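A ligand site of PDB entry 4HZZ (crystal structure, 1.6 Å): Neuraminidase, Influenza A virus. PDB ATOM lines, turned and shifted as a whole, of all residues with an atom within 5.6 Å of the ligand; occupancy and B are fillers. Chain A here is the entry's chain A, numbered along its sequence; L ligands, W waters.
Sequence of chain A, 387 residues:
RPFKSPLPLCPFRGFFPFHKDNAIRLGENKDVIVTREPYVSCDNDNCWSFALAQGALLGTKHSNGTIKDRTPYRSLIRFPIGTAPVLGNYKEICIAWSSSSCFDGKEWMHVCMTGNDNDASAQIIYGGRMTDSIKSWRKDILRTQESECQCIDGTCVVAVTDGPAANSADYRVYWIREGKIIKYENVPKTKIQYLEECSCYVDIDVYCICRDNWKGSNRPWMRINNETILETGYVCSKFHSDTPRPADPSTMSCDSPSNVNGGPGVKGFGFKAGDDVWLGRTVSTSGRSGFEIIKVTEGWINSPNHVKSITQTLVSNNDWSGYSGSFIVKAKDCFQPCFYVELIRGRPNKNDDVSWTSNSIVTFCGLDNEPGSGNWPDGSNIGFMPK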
ATOM      1  N   ARG A  36      31.753  21.592   7.972  1.00  0.00           N
ATOM      2  CA  ARG A  36      31.246  20.657   8.972  1.00  0.00           C
ATOM      3  C   ARG A  36      31.523  19.252   8.434  1.00  0.00           C
ATOM      4  O   ARG A  36      32.052  19.095   7.333  1.00  0.00           O
ATOM      5  CB  ARG A  36      29.753  20.850   9.318  1.00  0.00           C
ATOM      6  CG  ARG A  36      29.499  21.529  10.685  1.00  0.00           C
ATOM      7  CD  ARG A  36      28.213  20.984  11.329  1.00  0.00           C
ATOM      8  NE  ARG A  36      28.406  19.594  11.764  1.00  0.00           N
ATOM      9  CZ  ARG A  36      27.426  18.717  11.973  1.00  0.00           C
ATOM     10  NH1 ARG A  36      26.163  19.048  11.771  1.00  0.00           N
ATOM     11  NH2 ARG A  36      27.723  17.476  12.362  1.00  0.00           N
ATOM     12  N   GLU A  37      31.201  18.234   9.231  1.00  0.00           N
ATOM     13  CA  GLU A  37      31.420  16.844   8.831  1.00  0.00           C
ATOM     14  C   GLU A  37      32.864  16.574   8.420  1.00  0.00           C
ATOM     15  O   GLU A  37      33.143  16.039   7.331  1.00  0.00           O
ATOM     16  CB  GLU A  37      30.452  16.435   7.709  1.00  0.00           C
ATOM     17  CG  GLU A  37      28.981  16.509   8.125  1.00  0.00           C
ATOM     18  CD  GLU A  37      28.341  17.868   7.891  1.00  0.00           C
ATOM     19  OE1 GLU A  37      28.879  18.686   7.112  1.00  0.00           O
ATOM     20  OE2 GLU A  37      27.271  18.122   8.468  1.00  0.00           O
ATOM     21  N   ASP A  69      22.118  21.920   5.798  1.00  0.00           N
ATOM     22  CA  ASP A  69      22.935  20.747   5.472  1.00  0.00           C
ATOM     23  C   ASP A  69      23.350  20.629   4.013  1.00  0.00           C
ATOM     24  O   ASP A  69      24.503  20.313   3.718  1.00  0.00           O
ATOM     25  CB  ASP A  69      22.181  19.457   5.848  1.00  0.00           C
ATOM     26  CG  ASP A  69      22.114  19.247   7.343  1.00  0.00           C
ATOM     27  OD1 ASP A  69      23.188  19.307   7.985  1.00  0.00           O
ATOM     28  OD2 ASP A  69      21.002  19.010   7.857  1.00  0.00           O
ATOM     29  N   ARG A  70      22.428  20.877   3.097  1.00  0.00           N
ATOM     30  CA  ARG A  70      22.697  20.551   1.700  1.00  0.00           C
ATOM     31  C   ARG A  70      22.498  21.783   0.793  1.00  0.00           C
ATOM     32  O   ARG A  70      21.395  22.310   0.689  1.00  0.00           O
ATOM     33  CB  ARG A  70      21.812  19.365   1.267  1.00  0.00           C
ATOM     34  CG  ARG A  70      22.074  18.108   2.118  1.00  0.00           C
ATOM     35  CD  ARG A  70      21.142  16.925   1.754  1.00  0.00           C
ATOM     36  NE  ARG A  70      19.745  17.289   1.939  1.00  0.00           N
ATOM     37  CZ  ARG A  70      19.127  17.326   3.125  1.00  0.00           C
ATOM     38  NH1 ARG A  70      17.848  17.698   3.178  1.00  0.00           N
ATOM     39  NH2 ARG A  70      19.772  17.015   4.244  1.00  0.00           N
ATOM     40  N   ARG A  74      28.520  23.443  -1.393  1.00  0.00           N
ATOM     41  CA  ARG A  74      29.359  22.585  -0.562  1.00  0.00           C
ATOM     42  C   ARG A  74      30.249  21.712  -1.422  1.00  0.00           C
ATOM     43  O   ARG A  74      29.822  21.152  -2.435  1.00  0.00           O
ATOM     44  CB  ARG A  74      28.496  21.728   0.383  1.00  0.00           C
ATOM     45  CG  ARG A  74      27.589  22.556   1.292  1.00  0.00           C
ATOM     46  CD  ARG A  74      27.180  21.746   2.517  1.00  0.00           C
ATOM     47  NE  ARG A  74      28.274  21.646   3.485  1.00  0.00           N
ATOM     48  CZ  ARG A  74      28.121  21.151   4.707  1.00  0.00           C
ATOM     49  NH1 ARG A  74      26.926  20.721   5.083  1.00  0.00           N
ATOM     50  NH2 ARG A  74      29.153  21.114   5.560  1.00  0.00           N
ATOM     51  N   TRP A  97      27.745  17.386  -0.691  1.00  0.00           N
ATOM     52  CA  TRP A  97      27.182  17.625   0.629  1.00  0.00           C
ATOM     53  C   TRP A  97      27.101  16.372   1.500  1.00  0.00           C
ATOM     54  O   TRP A  97      26.523  16.391   2.585  1.00  0.00           O
ATOM     55  CB  TRP A  97      25.831  18.390   0.579  1.00  0.00           C
ATOM     56  CG  TRP A  97      24.801  17.945  -0.439  1.00  0.00           C
ATOM     57  CD1 TRP A  97      24.305  18.680  -1.475  1.00  0.00           C
ATOM     58  CD2 TRP A  97      24.100  16.678  -0.490  1.00  0.00           C
ATOM     59  NE1 TRP A  97      23.363  17.961  -2.180  1.00  0.00           N
ATOM     60  CE2 TRP A  97      23.229  16.730  -1.601  1.00  0.00           C
ATOM     61  CE3 TRP A  97      24.157  15.509   0.273  1.00  0.00           C
ATOM     62  CZ2 TRP A  97      22.397  15.665  -1.948  1.00  0.00           C
ATOM     63  CZ3 TRP A  97      23.325  14.444  -0.073  1.00  0.00           C
ATOM     64  CH2 TRP A  97      22.457  14.524  -1.186  1.00  0.00           C
ATOM     65  N   SER A  98      27.697  15.284   1.012  1.00  0.00           N
ATOM     66  CA  SER A  98      27.946  14.075   1.799  1.00  0.00           C
ATOM     67  C   SER A  98      29.128  13.389   1.128  1.00  0.00           C
ATOM     68  O   SER A  98      29.224  13.407  -0.096  1.00  0.00           O
ATOM     69  CB  SER A  98      26.720  13.163   1.826  1.00  0.00           C
ATOM     70  OG  SER A  98      26.955  12.036   2.661  1.00  0.00           O
ATOM     71  N   ILE A 141      17.708  11.873  -0.604  1.00  0.00           N
ATOM     72  CA  ILE A 141      18.996  12.187   0.026  1.00  0.00           C
ATOM     73  C   ILE A 141      19.978  11.010   0.024  1.00  0.00           C
ATOM     74  O   ILE A 141      20.407  10.518   1.072  1.00  0.00           O
ATOM     75  CB  ILE A 141      18.824  12.768   1.444  1.00  0.00           C
ATOM     76  CG1 ILE A 141      17.692  13.791   1.464  1.00  0.00           C
ATOM     77  CG2 ILE A 141      20.121  13.418   1.901  1.00  0.00           C
ATOM     78  CD1 ILE A 141      17.347  14.282   2.867  1.00  0.00           C
ATOM     79  N   ARG A 143      23.292   9.360   0.269  1.00  0.00           N
ATOM     80  CA  ARG A 143      24.247   9.854   1.267  1.00  0.00           C
ATOM     81  C   ARG A 143      25.223   8.774   1.746  1.00  0.00           C
ATOM     82  O   ARG A 143      24.978   7.578   1.585  1.00  0.00           O
ATOM     83  CB  ARG A 143      23.479  10.436   2.466  1.00  0.00           C
ATOM     84  CG  ARG A 143      22.583   9.419   3.188  1.00  0.00           C
ATOM     85  CD  ARG A 143      21.559  10.130   4.079  1.00  0.00           C
ATOM     86  NE  ARG A 143      20.633   9.213   4.762  1.00  0.00           N
ATOM     87  CZ  ARG A 143      19.433   8.866   4.302  1.00  0.00           C
ATOM     88  NH1 ARG A 143      18.991   9.338   3.140  1.00  0.00           N
ATOM     89  NH2 ARG A 143      18.668   8.040   5.007  1.00  0.00           N
ATOM     90  N   GLU A 146      30.560  10.177   5.797  1.00  0.00           N
ATOM     91  CA  GLU A 146      31.192  11.352   6.406  1.00  0.00           C
ATOM     92  C   GLU A 146      32.456  10.981   7.203  1.00  0.00           C
ATOM     93  O   GLU A 146      32.826  11.698   8.123  1.00  0.00           O
ATOM     94  CB  GLU A 146      30.236  12.156   7.299  1.00  0.00           C
ATOM     95  CG  GLU A 146      28.783  12.206   6.837  1.00  0.00           C
ATOM     96  CD  GLU A 146      28.552  12.893   5.495  1.00  0.00           C
ATOM     97  OE1 GLU A 146      29.511  13.314   4.808  1.00  0.00           O
ATOM     98  OE2 GLU A 146      27.366  13.006   5.127  1.00  0.00           O
ATOM     99  N   ALA A 165      15.020   9.516   5.918  1.00  0.00           N
ATOM    100  CA  ALA A 165      15.434   9.604   7.313  1.00  0.00           C
ATOM    101  C   ALA A 165      14.148   9.718   8.123  1.00  0.00           C
ATOM    102  O   ALA A 165      13.556  10.800   8.206  1.00  0.00           O
ATOM    103  CB  ALA A 165      16.330  10.817   7.531  1.00  0.00           C
ATOM    104  N   GLU A 196      23.048   4.819   9.781  1.00  0.00           N
ATOM    105  CA  GLU A 196      23.525   6.044   9.134  1.00  0.00           C
ATOM    106  C   GLU A 196      24.982   6.284   9.463  1.00  0.00           C
ATOM    107  O   GLU A 196      25.472   5.870  10.506  1.00  0.00           O
ATOM    108  CB  GLU A 196      22.703   7.241   9.622  1.00  0.00           C
ATOM    109  CG  GLU A 196      21.196   7.140   9.366  1.00  0.00           C
ATOM    110  CD  GLU A 196      20.809   7.495   7.922  1.00  0.00           C
ATOM    111  OE1 GLU A 196      19.641   7.242   7.550  1.00  0.00           O
ATOM    112  OE2 GLU A 196      21.657   8.017   7.167  1.00  0.00           O
ATOM    113  N   GLU A 197      25.692   6.960   8.562  1.00  0.00           N
ATOM    114  CA  GLU A 197      26.983   7.541   8.914  1.00  0.00           C
ATOM    115  C   GLU A 197      27.988   6.596   9.555  1.00  0.00           C
ATOM    116  O   GLU A 197      28.546   6.860  10.620  1.00  0.00           O
ATOM    117  CB  GLU A 197      26.771   8.782   9.794  1.00  0.00           C
ATOM    118  CG  GLU A 197      26.078   9.922   9.046  1.00  0.00           C
ATOM    119  CD  GLU A 197      25.700  11.076   9.944  1.00  0.00           C
ATOM    120  OE1 GLU A 197      25.589  10.861  11.164  1.00  0.00           O
ATOM    121  OE2 GLU A 197      25.497  12.197   9.416  1.00  0.00           O
ATOM    122  N   ARG A 211      25.272   4.819  13.205  1.00  0.00           N
ATOM    123  CA  ARG A 211      24.306   5.621  13.947  1.00  0.00           C
ATOM    124  C   ARG A 211      22.888   5.157  13.637  1.00  0.00           C
ATOM    125  O   ARG A 211      22.432   5.290  12.506  1.00  0.00           O
ATOM    126  CB  ARG A 211      24.476   7.095  13.553  1.00  0.00           C
ATOM    127  CG  ARG A 211      23.404   8.075  14.005  1.00  0.00           C
ATOM    128  CD  ARG A 211      23.629   9.439  13.316  1.00  0.00           C
ATOM    129  NE  ARG A 211      22.541  10.408  13.572  1.00  0.00           N
ATOM    130  CZ  ARG A 211      22.614  11.691  13.244  1.00  0.00           C
ATOM    131  NH1 ARG A 211      23.689  12.175  12.635  1.00  0.00           N
ATOM    132  NH2 ARG A 211      21.589  12.498  13.528  1.00  0.00           N
ATOM    133  N   ASN A 213      19.469   6.326  13.921  1.00  0.00           N
ATOM    134  CA  ASN A 213      18.919   7.649  14.173  1.00  0.00           C
ATOM    135  C   ASN A 213      17.456   7.645  14.606  1.00  0.00           C
ATOM    136  O   ASN A 213      16.819   8.679  14.647  1.00  0.00           O
ATOM    137  CB  ASN A 213      19.121   8.591  12.983  1.00  0.00           C
ATOM    138  CG  ASN A 213      18.311   8.179  11.751  1.00  0.00           C
ATOM    139  OD1 ASN A 213      17.832   9.046  11.010  1.00  0.00           O
ATOM    140  ND2 ASN A 213      18.162   6.892  11.536  1.00  0.00           N
ATOM    141  N   PRO A 264      17.972  12.011  17.855  1.00  0.00           N
ATOM    142  CA  PRO A 264      18.400  11.810  16.458  1.00  0.00           C
ATOM    143  C   PRO A 264      19.712  11.043  16.291  1.00  0.00           C
ATOM    144  O   PRO A 264      20.057  10.682  15.158  1.00  0.00           O
ATOM    145  CB  PRO A 264      18.602  13.246  15.968  1.00  0.00           C
ATOM    146  CG  PRO A 264      19.063  13.973  17.191  1.00  0.00           C
ATOM    147  CD  PRO A 264      18.238  13.387  18.319  1.00  0.00           C
ATOM    148  N   GLY A 265      20.436  10.806  17.381  1.00  0.00           N
ATOM    149  CA  GLY A 265      21.740  10.187  17.295  1.00  0.00           C
ATOM    150  C   GLY A 265      22.787  11.169  16.834  1.00  0.00           C
ATOM    151  O   GLY A 265      22.498  12.330  16.548  1.00  0.00           O
ATOM    152  N   VAL A 266      24.025  10.688  16.771  1.00  0.00           N
ATOM    153  CA  VAL A 266      25.161  11.481  16.294  1.00  0.00           C
ATOM    154  C   VAL A 266      26.140  10.487  15.686  1.00  0.00           C
ATOM    155  O   VAL A 266      26.209   9.346  16.125  1.00  0.00           O
ATOM    156  CB  VAL A 266      25.803  12.313  17.453  1.00  0.00           C
ATOM    157  CG1 VAL A 266      26.483  11.407  18.479  1.00  0.00           C
ATOM    158  CG2 VAL A 266      26.792  13.354  16.922  1.00  0.00           C
ATOM    159  N   ARG A 288      25.147  17.392  22.365  1.00  0.00           N
ATOM    160  CA  ARG A 288      26.454  17.223  21.734  1.00  0.00           C
ATOM    161  C   ARG A 288      27.527  18.035  22.446  1.00  0.00           C
ATOM    162  O   ARG A 288      28.137  18.944  21.873  1.00  0.00           O
ATOM    163  CB  ARG A 288      26.350  17.573  20.251  1.00  0.00           C
ATOM    164  CG  ARG A 288      25.486  16.550  19.512  1.00  0.00           C
ATOM    165  CD  ARG A 288      25.194  16.982  18.088  1.00  0.00           C
ATOM    166  NE  ARG A 288      24.466  15.932  17.377  1.00  0.00           N
ATOM    167  CZ  ARG A 288      24.224  15.938  16.070  1.00  0.00           C
ATOM    168  NH1 ARG A 288      24.634  16.964  15.322  1.00  0.00           N
ATOM    169  NH2 ARG A 288      23.574  14.926  15.524  1.00  0.00           N
ATOM    170  N   TYR A 323      30.283  15.272  15.672  1.00  0.00           N
ATOM    171  CA  TYR A 323      30.610  13.993  15.065  1.00  0.00           C
ATOM    172  C   TYR A 323      31.977  13.466  15.509  1.00  0.00           C
ATOM    173  O   TYR A 323      32.855  14.216  15.917  1.00  0.00           O
ATOM    174  CB  TYR A 323      30.632  14.162  13.540  1.00  0.00           C
ATOM    175  CG  TYR A 323      29.266  14.135  12.895  1.00  0.00           C
ATOM    176  CD1 TYR A 323      28.107  14.289  13.654  1.00  0.00           C
ATOM    177  CD2 TYR A 323      29.137  13.947  11.532  1.00  0.00           C
ATOM    178  CE1 TYR A 323      26.842  14.239  13.060  1.00  0.00           C
ATOM    179  CE2 TYR A 323      27.873  13.903  10.925  1.00  0.00           C
ATOM    180  CZ  TYR A 323      26.741  14.041  11.702  1.00  0.00           C
ATOM    181  OH  TYR A 323      25.489  14.005  11.123  1.00  0.00           O
HETATM  182  C1  LIG L   1      23.510  16.039  12.122  1.00  0.00           C
HETATM  183  O1  LIG L   1      24.264  16.876  12.557  1.00  0.00           O
HETATM  184  O2  LIG L   1      22.786  15.170  12.896  1.00  0.00           O
HETATM  185  C2  LIG L   1      23.357  15.876  10.667  1.00  0.00           C
HETATM  186  C3  LIG L   1      24.175  16.743   9.693  1.00  0.00           C
HETATM  187  C4  LIG L   1      24.349  16.180   8.323  1.00  0.00           C
HETATM  188  C5  LIG L   1      23.309  15.217   7.768  1.00  0.00           C
HETATM  189  N1  LIG L   1      23.498  14.684   6.462  1.00  0.00           N
HETATM  190  C6  LIG L   1      23.021  15.264   5.264  1.00  0.00           C
HETATM  191  O3  LIG L   1      22.290  16.235   5.260  1.00  0.00           O
HETATM  192  C7  LIG L   1      23.403  14.543   4.003  1.00  0.00           C
HETATM  193  C8  LIG L   1      22.519  14.338   8.723  1.00  0.00           C
HETATM  194  C9  LIG L   1      22.583  14.642  10.217  1.00  0.00           C
HETATM  195  O4  LIG L   1      21.373  13.694   8.294  1.00  0.00           O
HETATM  196  C10 LIG L   1      21.481  12.396   7.790  1.00  0.00           C
HETATM  197  C11 LIG L   1      21.834  11.355   8.824  1.00  0.00           C
HETATM  198  C12 LIG L   1      20.243  12.093   6.979  1.00  0.00           C
HETATM  199  C13 LIG L   1      19.937  13.076   5.887  1.00  0.00           C
HETATM  200  C14 LIG L   1      20.834  11.128   9.920  1.00  0.00           C
HETATM  201  N2  LIG L   1      25.011  17.052   7.397  1.00  0.00           N
HETATM  202  O   HOH W   1      19.208  15.061   9.024  1.00  0.00           O
HETATM  203  O   HOH W   2      26.434  15.574   5.342  1.00  0.00           O
HETATM  204  O   HOH W   3      25.275  12.569   6.736  1.00  0.00           O
HETATM  205  O   HOH W   4      25.983  20.377   7.867  1.00  0.00           O
HETATM  206  O   HOH W   5      25.112  17.718   4.629  1.00  0.00           O
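NH2 of Arg 288 is in salt-bridge range of O2 of the ligand (2.8 Å).
N2 of the ligand lies within salt-bridge range of OE2 of Glu 37.
OD1 of Asp 69 is in salt-bridge range of N2 of the ligand (3.0 Å).
An oxygen (O3) of the ligand sits at hydrogen-bond distance from the guanidinium group of Arg 70, 2.8 Å away.
The guanidinium group of Arg 211 is in salt-bridge range of an oxygen (O2) of the ligand, 3.0 Å away.
An oxygen (O1) of the ligand is in salt-bridge range of the guanidinium group (NH1) of Arg 36.
The side-chain hydroxyl of Tyr 323 sits close to an oxygen (O1) of the ligand (3.4 Å).
OH of Tyr 323 sits at hydrogen-bond distance from NH1 of Arg 211 (3.0 Å).
OE2 of Glu 37 is in salt-bridge range of NH1 of Arg 36 (3.6 Å).
NH2 of Arg 143 lies within salt-bridge range of OE1 of Glu 196 (2.8 Å).
OE1 of Glu 37 is in salt-bridge range of NH2 of Arg 74 (2.9 Å).
NH2 of Arg 211 is in hydrogen-bond range of O of Gly 265, 3.2 Å away.
O of Asp 69 sits at hydrogen-bond distance from NH1 of Arg 74, at 2.8 Å.
NH1 of Arg 211 lies within salt-bridge range of OE1 of Glu 197 (2.7 Å).
NH2 of Arg 288 sits at hydrogen-bond distance from O of Gly 265, at 3.0 Å.
O of Trp 97 touches C7 of the ligand, 3.9 Å away.
Arg 143 touches the ligand.
Glu 196 touches the ligand (OE2 to C11, 3.7 Å).
Glu 197 touches the ligand (OE2 to C8, 3.7 Å).
Asn 213 touches the ligand.
Within 4 Å of the ligand: Arg 36, Glu 37, Asp 69, Arg 70, Trp 97, Arg 143, Glu 196, Glu 197, Arg 211, Asn 213, Arg 288 and Tyr 323.
Water W3 lies within hydrogen-bond range of the side-chain carboxylate (OE2) of Glu 146, the side-chain carboxylate (OE2) of Glu 197 and a nitrogen (N1) of the ligand.
Water W5 lies within hydrogen-bond range of O of Trp 97 (2.8 Å), O of Asp 69 (2.8 Å) and N2 of the ligand (2.8 Å).
Water W2 lies within hydrogen-bond range of the side-chain carboxylate (OE2) of Glu 146 (2.7 Å), the backbone carbonyl oxygen (O) of Trp 97 (2.9 Å) and a nitrogen (N2) of the ligand (2.9 Å).
Water W4 lies within hydrogen-bond range of the side-chain carboxylate of Glu 37 (2.7 Å), the guanidinium group of Arg 74 (3.0 Å), the side-chain carboxylate of Asp 69 (3.0 Å) and a nitrogen (N2) of the ligand (3.5 Å).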
